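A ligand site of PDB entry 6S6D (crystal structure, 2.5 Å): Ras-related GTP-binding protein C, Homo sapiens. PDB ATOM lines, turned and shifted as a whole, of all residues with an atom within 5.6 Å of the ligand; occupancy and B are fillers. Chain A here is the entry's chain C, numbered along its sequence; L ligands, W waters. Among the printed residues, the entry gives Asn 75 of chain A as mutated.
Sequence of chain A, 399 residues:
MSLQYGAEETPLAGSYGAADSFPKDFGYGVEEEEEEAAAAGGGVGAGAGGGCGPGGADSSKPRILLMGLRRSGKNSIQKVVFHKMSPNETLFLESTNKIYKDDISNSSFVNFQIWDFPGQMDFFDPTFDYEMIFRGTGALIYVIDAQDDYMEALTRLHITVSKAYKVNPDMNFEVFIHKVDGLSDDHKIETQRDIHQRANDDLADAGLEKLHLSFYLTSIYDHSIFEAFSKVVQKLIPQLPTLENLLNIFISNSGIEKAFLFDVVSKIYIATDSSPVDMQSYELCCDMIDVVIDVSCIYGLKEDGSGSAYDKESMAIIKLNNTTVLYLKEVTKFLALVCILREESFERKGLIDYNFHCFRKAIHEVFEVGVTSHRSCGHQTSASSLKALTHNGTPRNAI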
ATOM      1  N   GLY A  68       7.458  13.030 -39.155  1.00  0.00           N
ATOM      2  CA  GLY A  68       8.595  13.893 -38.755  1.00  0.00           C
ATOM      3  C   GLY A  68       9.788  13.125 -38.206  1.00  0.00           C
ATOM      4  O   GLY A  68       9.608  12.084 -37.580  1.00  0.00           O
ATOM      5  N   LEU A  69      10.998  13.637 -38.407  1.00  0.00           N
ATOM      6  CA  LEU A  69      12.235  13.102 -37.785  1.00  0.00           C
ATOM      7  C   LEU A  69      12.085  13.115 -36.258  1.00  0.00           C
ATOM      8  O   LEU A  69      11.256  13.882 -35.748  1.00  0.00           O
ATOM      9  CB  LEU A  69      13.439  13.938 -38.227  1.00  0.00           C
ATOM     10  CG  LEU A  69      13.564  14.162 -39.741  1.00  0.00           C
ATOM     11  CD1 LEU A  69      14.870  14.855 -40.095  1.00  0.00           C
ATOM     12  CD2 LEU A  69      13.396  12.864 -40.503  1.00  0.00           C
ATOM     13  N   ARG A  70      12.873  12.294 -35.561  1.00  0.00           N
ATOM     14  CA  ARG A  70      12.894  12.169 -34.080  1.00  0.00           C
ATOM     15  C   ARG A  70      13.332  13.524 -33.517  1.00  0.00           C
ATOM     16  O   ARG A  70      14.198  14.183 -34.123  1.00  0.00           O
ATOM     17  CB  ARG A  70      13.848  11.066 -33.608  1.00  0.00           C
ATOM     18  CG  ARG A  70      14.003   9.901 -34.574  1.00  0.00           C
ATOM     19  CD  ARG A  70      14.933   8.831 -34.059  1.00  0.00           C
ATOM     20  NE  ARG A  70      14.355   8.189 -32.883  1.00  0.00           N
ATOM     21  CZ  ARG A  70      14.736   7.034 -32.392  1.00  0.00           C
ATOM     22  NH1 ARG A  70      15.721   6.343 -32.953  1.00  0.00           N
ATOM     23  NH2 ARG A  70      14.114   6.551 -31.325  1.00  0.00           N
ATOM     24  N   ARG A  71      12.732  13.919 -32.391  1.00  0.00           N
ATOM     25  CA  ARG A  71      12.936  15.219 -31.700  1.00  0.00           C
ATOM     26  C   ARG A  71      12.280  16.365 -32.531  1.00  0.00           C
ATOM     27  O   ARG A  71      12.436  17.544 -32.112  1.00  0.00           O
ATOM     28  CB  ARG A  71      14.428  15.409 -31.353  1.00  0.00           C
ATOM     29  CG  ARG A  71      14.973  14.451 -30.282  1.00  0.00           C
ATOM     30  CD  ARG A  71      16.504  14.284 -30.259  1.00  0.00           C
ATOM     31  N   SER A  72      11.562  16.079 -33.640  1.00  0.00           N
ATOM     32  CA  SER A  72      10.753  17.123 -34.344  1.00  0.00           C
ATOM     33  C   SER A  72       9.670  17.636 -33.385  1.00  0.00           C
ATOM     34  O   SER A  72       9.622  18.842 -33.183  1.00  0.00           O
ATOM     35  CB  SER A  72      10.205  16.678 -35.670  1.00  0.00           C
ATOM     36  OG  SER A  72       9.220  15.684 -35.546  1.00  0.00           O
ATOM     37  N   GLY A  73       8.975  16.730 -32.693  1.00  0.00           N
ATOM     38  CA  GLY A  73       8.147  17.036 -31.500  1.00  0.00           C
ATOM     39  C   GLY A  73       6.790  16.344 -31.530  1.00  0.00           C
ATOM     40  O   GLY A  73       5.896  16.818 -30.819  1.00  0.00           O
ATOM     41  N   LYS A  74       6.669  15.253 -32.283  1.00  0.00           N
ATOM     42  CA  LYS A  74       5.438  14.477 -32.550  1.00  0.00           C
ATOM     43  C   LYS A  74       4.773  14.066 -31.245  1.00  0.00           C
ATOM     44  O   LYS A  74       3.578  14.258 -31.098  1.00  0.00           O
ATOM     45  CB  LYS A  74       5.775  13.188 -33.302  1.00  0.00           C
ATOM     46  CG  LYS A  74       6.319  13.385 -34.709  1.00  0.00           C
ATOM     47  CD  LYS A  74       6.634  12.067 -35.383  1.00  0.00           C
ATOM     48  CE  LYS A  74       7.979  11.497 -34.997  1.00  0.00           C
ATOM     49  NZ  LYS A  74       8.358  10.394 -35.901  1.00  0.00           N
ATOM     50  N   ASN A  75       5.536  13.459 -30.352  1.00  0.00           N
ATOM     51  CA  ASN A  75       4.984  12.915 -29.084  1.00  0.00           C
ATOM     52  C   ASN A  75       4.441  14.097 -28.289  1.00  0.00           C
ATOM     53  O   ASN A  75       3.395  13.956 -27.654  1.00  0.00           O
ATOM     54  CB  ASN A  75       6.023  12.078 -28.322  1.00  0.00           C
ATOM     55  CG  ASN A  75       5.370  11.100 -27.366  1.00  0.00           C
ATOM     56  OD1 ASN A  75       5.474  11.251 -26.143  1.00  0.00           O
ATOM     57  ND2 ASN A  75       4.678  10.121 -27.923  1.00  0.00           N
ATOM     58  N   SER A  76       5.151  15.223 -28.341  1.00  0.00           N
ATOM     59  CA  SER A  76       4.826  16.460 -27.593  1.00  0.00           C
ATOM     60  C   SER A  76       3.511  17.058 -28.118  1.00  0.00           C
ATOM     61  O   SER A  76       2.726  17.495 -27.289  1.00  0.00           O
ATOM     62  CB  SER A  76       5.964  17.424 -27.668  1.00  0.00           C
ATOM     63  OG  SER A  76       7.184  16.783 -27.327  1.00  0.00           O
ATOM     64  N   ILE A  77       3.277  16.999 -29.426  1.00  0.00           N
ATOM     65  CA  ILE A  77       2.054  17.504 -30.105  1.00  0.00           C
ATOM     66  C   ILE A  77       0.887  16.581 -29.711  1.00  0.00           C
ATOM     67  O   ILE A  77      -0.138  17.079 -29.168  1.00  0.00           O
ATOM     68  CB  ILE A  77       2.327  17.666 -31.636  1.00  0.00           C
ATOM     69  CG1 ILE A  77       3.351  18.789 -31.900  1.00  0.00           C
ATOM     70  CG2 ILE A  77       1.056  17.904 -32.419  1.00  0.00           C
ATOM     71  CD1 ILE A  77       3.829  18.915 -33.340  1.00  0.00           C
ATOM     72  N   PRO A  87       2.537  21.053 -21.611  1.00  0.00           N
ATOM     73  CA  PRO A  87       3.685  20.981 -22.520  1.00  0.00           C
ATOM     74  C   PRO A  87       5.026  20.539 -21.905  1.00  0.00           C
ATOM     75  O   PRO A  87       5.738  19.754 -22.545  1.00  0.00           O
ATOM     76  CB  PRO A  87       3.797  22.424 -23.038  1.00  0.00           C
ATOM     77  CG  PRO A  87       3.162  23.264 -21.942  1.00  0.00           C
ATOM     78  CD  PRO A  87       2.020  22.418 -21.445  1.00  0.00           C
ATOM     79  N   THR A  90       6.197  16.758 -21.394  1.00  0.00           N
ATOM     80  CA  THR A  90       6.553  16.054 -22.666  1.00  0.00           C
ATOM     81  C   THR A  90       8.087  15.969 -22.838  1.00  0.00           C
ATOM     82  O   THR A  90       8.543  15.316 -23.816  1.00  0.00           O
ATOM     83  CB  THR A  90       5.964  16.726 -23.924  1.00  0.00           C
ATOM     84  OG1 THR A  90       6.646  17.954 -24.162  1.00  0.00           O
ATOM     85  CG2 THR A  90       4.476  17.002 -23.849  1.00  0.00           C
ATOM     86  N   LEU A  91       8.870  16.591 -21.942  1.00  0.00           N
ATOM     87  CA  LEU A  91      10.365  16.490 -21.903  1.00  0.00           C
ATOM     88  C   LEU A  91      10.794  15.073 -21.480  1.00  0.00           C
ATOM     89  O   LEU A  91      12.002  14.776 -21.607  1.00  0.00           O
ATOM     90  CB  LEU A  91      10.951  17.546 -20.950  1.00  0.00           C
ATOM     91  CG  LEU A  91      11.486  18.813 -21.621  1.00  0.00           C
ATOM     92  CD1 LEU A  91      11.625  19.962 -20.639  1.00  0.00           C
ATOM     93  CD2 LEU A  91      12.822  18.542 -22.300  1.00  0.00           C
ATOM     94  N   LEU A  93       9.085  11.614 -22.563  1.00  0.00           N
ATOM     95  CA  LEU A  93       8.167  10.704 -23.316  1.00  0.00           C
ATOM     96  C   LEU A  93       8.820  10.276 -24.635  1.00  0.00           C
ATOM     97  O   LEU A  93       9.529   9.250 -24.602  1.00  0.00           O
ATOM     98  CB  LEU A  93       6.842  11.437 -23.572  1.00  0.00           C
ATOM     99  N   ILE A 114       0.386   9.175 -34.803  1.00  0.00           N
ATOM    100  CA  ILE A 114       1.859   9.275 -35.081  1.00  0.00           C
ATOM    101  C   ILE A 114       2.305   8.105 -35.978  1.00  0.00           C
ATOM    102  O   ILE A 114       1.689   7.021 -35.881  1.00  0.00           O
ATOM    103  CB  ILE A 114       2.642   9.267 -33.743  1.00  0.00           C
ATOM    104  CG1 ILE A 114       2.600  10.630 -33.041  1.00  0.00           C
ATOM    105  CG2 ILE A 114       4.063   8.773 -33.963  1.00  0.00           C
ATOM    106  CD1 ILE A 114       3.583  10.773 -31.880  1.00  0.00           C
ATOM    107  N   GLN A 147      13.984  25.120 -34.445  1.00  0.00           N
ATOM    108  CA  GLN A 147      15.123  25.384 -33.528  1.00  0.00           C
ATOM    109  C   GLN A 147      16.354  24.675 -34.112  1.00  0.00           C
ATOM    110  O   GLN A 147      17.472  25.088 -33.766  1.00  0.00           O
ATOM    111  CB  GLN A 147      14.822  24.921 -32.093  1.00  0.00           C
ATOM    112  CG  GLN A 147      13.700  25.681 -31.416  1.00  0.00           C
ATOM    113  CD  GLN A 147      13.926  25.975 -29.960  1.00  0.00           C
ATOM    114  OE1 GLN A 147      14.958  26.522 -29.588  1.00  0.00           O
ATOM    115  NE2 GLN A 147      12.959  25.661 -29.117  1.00  0.00           N
ATOM    116  N   HIS A 178       7.639  23.661 -36.423  1.00  0.00           N
ATOM    117  CA  HIS A 178       7.305  23.473 -34.990  1.00  0.00           C
ATOM    118  C   HIS A 178       8.465  24.043 -34.173  1.00  0.00           C
ATOM    119  O   HIS A 178       9.495  24.368 -34.789  1.00  0.00           O
ATOM    120  CB  HIS A 178       6.836  22.009 -34.768  1.00  0.00           C
ATOM    121  CG  HIS A 178       6.552  21.709 -33.333  1.00  0.00           C
ATOM    122  ND1 HIS A 178       5.496  22.280 -32.666  1.00  0.00           N
ATOM    123  CD2 HIS A 178       7.239  20.980 -32.421  1.00  0.00           C
ATOM    124  CE1 HIS A 178       5.531  21.907 -31.395  1.00  0.00           C
ATOM    125  NE2 HIS A 178       6.600  21.112 -31.223  1.00  0.00           N
ATOM    126  N   LYS A 179       8.211  24.324 -32.889  1.00  0.00           N
ATOM    127  CA  LYS A 179       9.141  24.811 -31.836  1.00  0.00           C
ATOM    128  C   LYS A 179       9.539  26.292 -32.064  1.00  0.00           C
ATOM    129  O   LYS A 179      10.644  26.688 -31.615  1.00  0.00           O
ATOM    130  CB  LYS A 179      10.378  23.916 -31.736  1.00  0.00           C
ATOM    131  CG  LYS A 179      10.125  22.415 -31.633  1.00  0.00           C
ATOM    132  CD  LYS A 179      11.236  21.728 -30.861  1.00  0.00           C
ATOM    133  CE  LYS A 179      11.477  20.274 -31.215  1.00  0.00           C
ATOM    134  NZ  LYS A 179      12.729  19.772 -30.588  1.00  0.00           N
ATOM    135  N   VAL A 180       8.656  27.100 -32.647  1.00  0.00           N
ATOM    136  CA  VAL A 180       9.011  28.510 -33.007  1.00  0.00           C
ATOM    137  C   VAL A 180       8.991  29.370 -31.742  1.00  0.00           C
ATOM    138  O   VAL A 180       9.420  30.489 -31.837  1.00  0.00           O
ATOM    139  CB  VAL A 180       8.144  29.107 -34.121  1.00  0.00           C
ATOM    140  CG1 VAL A 180       8.077  28.185 -35.342  1.00  0.00           C
ATOM    141  CG2 VAL A 180       6.746  29.459 -33.630  1.00  0.00           C
ATOM    142  N   ASP A 181       8.584  28.834 -30.580  1.00  0.00           N
ATOM    143  CA  ASP A 181       8.620  29.578 -29.289  1.00  0.00           C
ATOM    144  C   ASP A 181      10.048  29.863 -28.798  1.00  0.00           C
ATOM    145  O   ASP A 181      10.186  30.634 -27.812  1.00  0.00           O
ATOM    146  CB  ASP A 181       7.877  28.838 -28.172  1.00  0.00           C
ATOM    147  CG  ASP A 181       8.572  27.546 -27.813  1.00  0.00           C
ATOM    148  OD1 ASP A 181       8.326  26.554 -28.542  1.00  0.00           O
ATOM    149  OD2 ASP A 181       9.426  27.563 -26.899  1.00  0.00           O
ATOM    150  N   GLY A 182      11.066  29.239 -29.403  1.00  0.00           N
ATOM    151  CA  GLY A 182      12.488  29.453 -29.082  1.00  0.00           C
ATOM    152  C   GLY A 182      13.141  30.480 -29.988  1.00  0.00           C
ATOM    153  O   GLY A 182      14.315  30.841 -29.737  1.00  0.00           O
ATOM    154  N   THR A 218       3.655  26.641 -35.201  1.00  0.00           N
ATOM    155  CA  THR A 218       3.037  25.879 -34.079  1.00  0.00           C
ATOM    156  C   THR A 218       3.939  25.944 -32.859  1.00  0.00           C
ATOM    157  O   THR A 218       5.108  26.273 -32.993  1.00  0.00           O
ATOM    158  CB  THR A 218       2.813  24.442 -34.525  1.00  0.00           C
ATOM    159  OG1 THR A 218       4.138  23.923 -34.674  1.00  0.00           O
ATOM    160  CG2 THR A 218       2.032  24.331 -35.825  1.00  0.00           C
ATOM    161  N   SER A 219       3.384  25.631 -31.698  1.00  0.00           N
ATOM    162  CA  SER A 219       4.171  25.510 -30.440  1.00  0.00           C
ATOM    163  C   SER A 219       3.267  24.930 -29.348  1.00  0.00           C
ATOM    164  O   SER A 219       2.121  25.364 -29.192  1.00  0.00           O
ATOM    165  CB  SER A 219       4.825  26.816 -30.038  1.00  0.00           C
ATOM    166  OG  SER A 219       5.173  26.781 -28.662  1.00  0.00           O
ATOM    167  N   ILE A 220       3.777  23.912 -28.663  1.00  0.00           N
ATOM    168  CA  ILE A 220       3.074  23.242 -27.544  1.00  0.00           C
ATOM    169  C   ILE A 220       2.911  24.264 -26.426  1.00  0.00           C
ATOM    170  O   ILE A 220       2.044  24.050 -25.560  1.00  0.00           O
ATOM    171  CB  ILE A 220       3.836  21.966 -27.086  1.00  0.00           C
ATOM    172  CG1 ILE A 220       5.236  22.270 -26.553  1.00  0.00           C
ATOM    173  CG2 ILE A 220       3.900  20.915 -28.187  1.00  0.00           C
ATOM    174  CD1 ILE A 220       5.855  21.086 -25.830  1.00  0.00           C
ATOM    175  N   TYR A 221       3.722  25.336 -26.416  1.00  0.00           N
ATOM    176  CA  TYR A 221       3.717  26.384 -25.367  1.00  0.00           C
ATOM    177  C   TYR A 221       2.756  27.527 -25.758  1.00  0.00           C
ATOM    178  O   TYR A 221       2.541  28.400 -24.921  1.00  0.00           O
ATOM    179  CB  TYR A 221       5.156  26.873 -25.116  1.00  0.00           C
ATOM    180  CG  TYR A 221       6.066  25.846 -24.482  1.00  0.00           C
ATOM    181  CD1 TYR A 221       6.010  25.612 -23.112  1.00  0.00           C
ATOM    182  CD2 TYR A 221       6.985  25.120 -25.216  1.00  0.00           C
ATOM    183  CE1 TYR A 221       6.829  24.680 -22.506  1.00  0.00           C
ATOM    184  CE2 TYR A 221       7.816  24.178 -24.626  1.00  0.00           C
ATOM    185  CZ  TYR A 221       7.731  23.951 -23.257  1.00  0.00           C
ATOM    186  OH  TYR A 221       8.538  23.028 -22.634  1.00  0.00           O
HETATM  187  P1  LIG L   1       9.355  13.116 -31.291  1.00  0.00           P
HETATM  188  O1  LIG L   1       8.353  12.396 -30.434  1.00  0.00           O
HETATM  189  O2  LIG L   1      10.668  12.344 -31.070  1.00  0.00           O
HETATM  190  O3  LIG L   1       9.037  13.194 -32.797  1.00  0.00           O
HETATM  191  O4  LIG L   1       9.758  14.509 -30.592  1.00  0.00           O
HETATM  192  P2  LIG L   1       9.387  14.484 -29.041  1.00  0.00           P
HETATM  193  O5  LIG L   1       7.905  14.763 -29.060  1.00  0.00           O
HETATM  194  O6  LIG L   1       9.782  13.187 -28.357  1.00  0.00           O
HETATM  195  O7  LIG L   1      10.035  15.639 -28.164  1.00  0.00           O
HETATM  196  C1  LIG L   1      10.817  16.635 -28.741  1.00  0.00           C
HETATM  197  C2  LIG L   1      11.691  17.280 -27.684  1.00  0.00           C
HETATM  198  O8  LIG L   1      11.546  18.635 -28.017  1.00  0.00           O
HETATM  199  C3  LIG L   1      11.307  17.254 -26.201  1.00  0.00           C
HETATM  200  O9  LIG L   1      12.361  17.835 -25.426  1.00  0.00           O
HETATM  201  C4  LIG L   1      10.210  18.260 -26.092  1.00  0.00           C
HETATM  202  O10 LIG L   1      10.151  18.918 -24.833  1.00  0.00           O
HETATM  203  C5  LIG L   1      10.701  19.291 -27.080  1.00  0.00           C
HETATM  204  N1  LIG L   1       9.607  19.965 -27.803  1.00  0.00           N
HETATM  205  C6  LIG L   1       8.585  19.440 -28.526  1.00  0.00           C
HETATM  206  N2  LIG L   1       7.821  20.428 -29.038  1.00  0.00           N
HETATM  207  C7  LIG L   1       8.367  21.592 -28.630  1.00  0.00           C
HETATM  208  C8  LIG L   1       8.078  23.023 -28.807  1.00  0.00           C
HETATM  209  O11 LIG L   1       7.090  23.416 -29.479  1.00  0.00           O
HETATM  210  N3  LIG L   1       8.920  23.885 -28.210  1.00  0.00           N
HETATM  211  C9  LIG L   1      10.004  23.511 -27.492  1.00  0.00           C
HETATM  212  N4  LIG L   1      10.811  24.441 -26.921  1.00  0.00           N
HETATM  213  N5  LIG L   1      10.309  22.213 -27.292  1.00  0.00           N
HETATM  214  C10 LIG L   1       9.531  21.261 -27.830  1.00  0.00           C
HETATM  215  O   HOH W   1      12.081  12.077 -28.657  1.00  0.00           O
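NE2 of His 178 lies within hydrogen-bond range of N2 of the ligand, at 2.6 Å. A nitrogen (N3) of the ligand lies within hydrogen-bond range of the side-chain carboxylate (OD1) of Asp 181 (2.8 Å). N of Ser 76 is in hydrogen-bond range of O5 of the ligand, 2.9 Å away. The side-chain hydroxyl (OG) of Ser 76 sits at hydrogen-bond distance from an oxygen (O5) of the ligand, at 2.8 Å. An oxygen (O2) of the ligand lies within hydrogen-bond range of the backbone NH of Arg 71, 2.9 Å away. O3 of the ligand lies close to N of Lys 74, 3.2 Å away. The backbone NH (N) of Asn 75 is in hydrogen-bond range of an oxygen (O5) of the ligand. An oxygen (O8) of the ligand lies within hydrogen-bond range of the side-chain amino group (NZ) of Lys 179 (3.0 Å). The backbone NH (N) of Gly 73 sits close to an oxygen (O4) of the ligand (3.2 Å). A nitrogen (N4) of the ligand lies close to the side-chain amide nitrogen (NE2) of Gln 147, at 3.3 Å. An oxygen (O11) of the ligand sits at hydrogen-bond distance from the backbone NH of Ile 220.
Merely in contact with the ligand: Leu 69 (3.8 Å), Arg 70 (3.7 Å), Ser 72 (3.7 Å), Thr 90 (3.7 Å), Leu 91 (3.2 Å), Ser 219 (3.7 Å) and Tyr 221 (3.7 Å). Of the 25 residues printed, 17 come within 4 Å of the ligand. The nearest printed residue that does not touch the ligand is Leu 93 (4.8 Å).
A ring nitrogen (ND1) of His 178 lies within hydrogen-bond range of the side-chain hydroxyl of Thr 218, 2.9 Å away. The side-chain carboxylate of Asp 181 is in hydrogen-bond range of the side-chain hydroxyl of Ser 219. The side-chain hydroxyl (OG) of Ser 76 is in hydrogen-bond range of the side-chain hydroxyl (OG1) of Thr 90 (3.4 Å). The backbone carbonyl oxygen (O) of Arg 71 is in hydrogen-bond range of the side-chain amino group (NZ) of Lys 179, 2.7 Å away. O of Gly 68 sits at hydrogen-bond distance from NZ of Lys 74. N of Tyr 221 lies close to OG of Ser 219, at 3.0 Å. The backbone carbonyl oxygen (O) of Pro 87 lies within hydrogen-bond range of the side-chain hydroxyl (OG1) of Thr 90 (2.6 Å). The side-chain hydroxyl of Ser 72 is in hydrogen-bond range of the backbone carbonyl oxygen of Leu 69 (2.7 Å).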
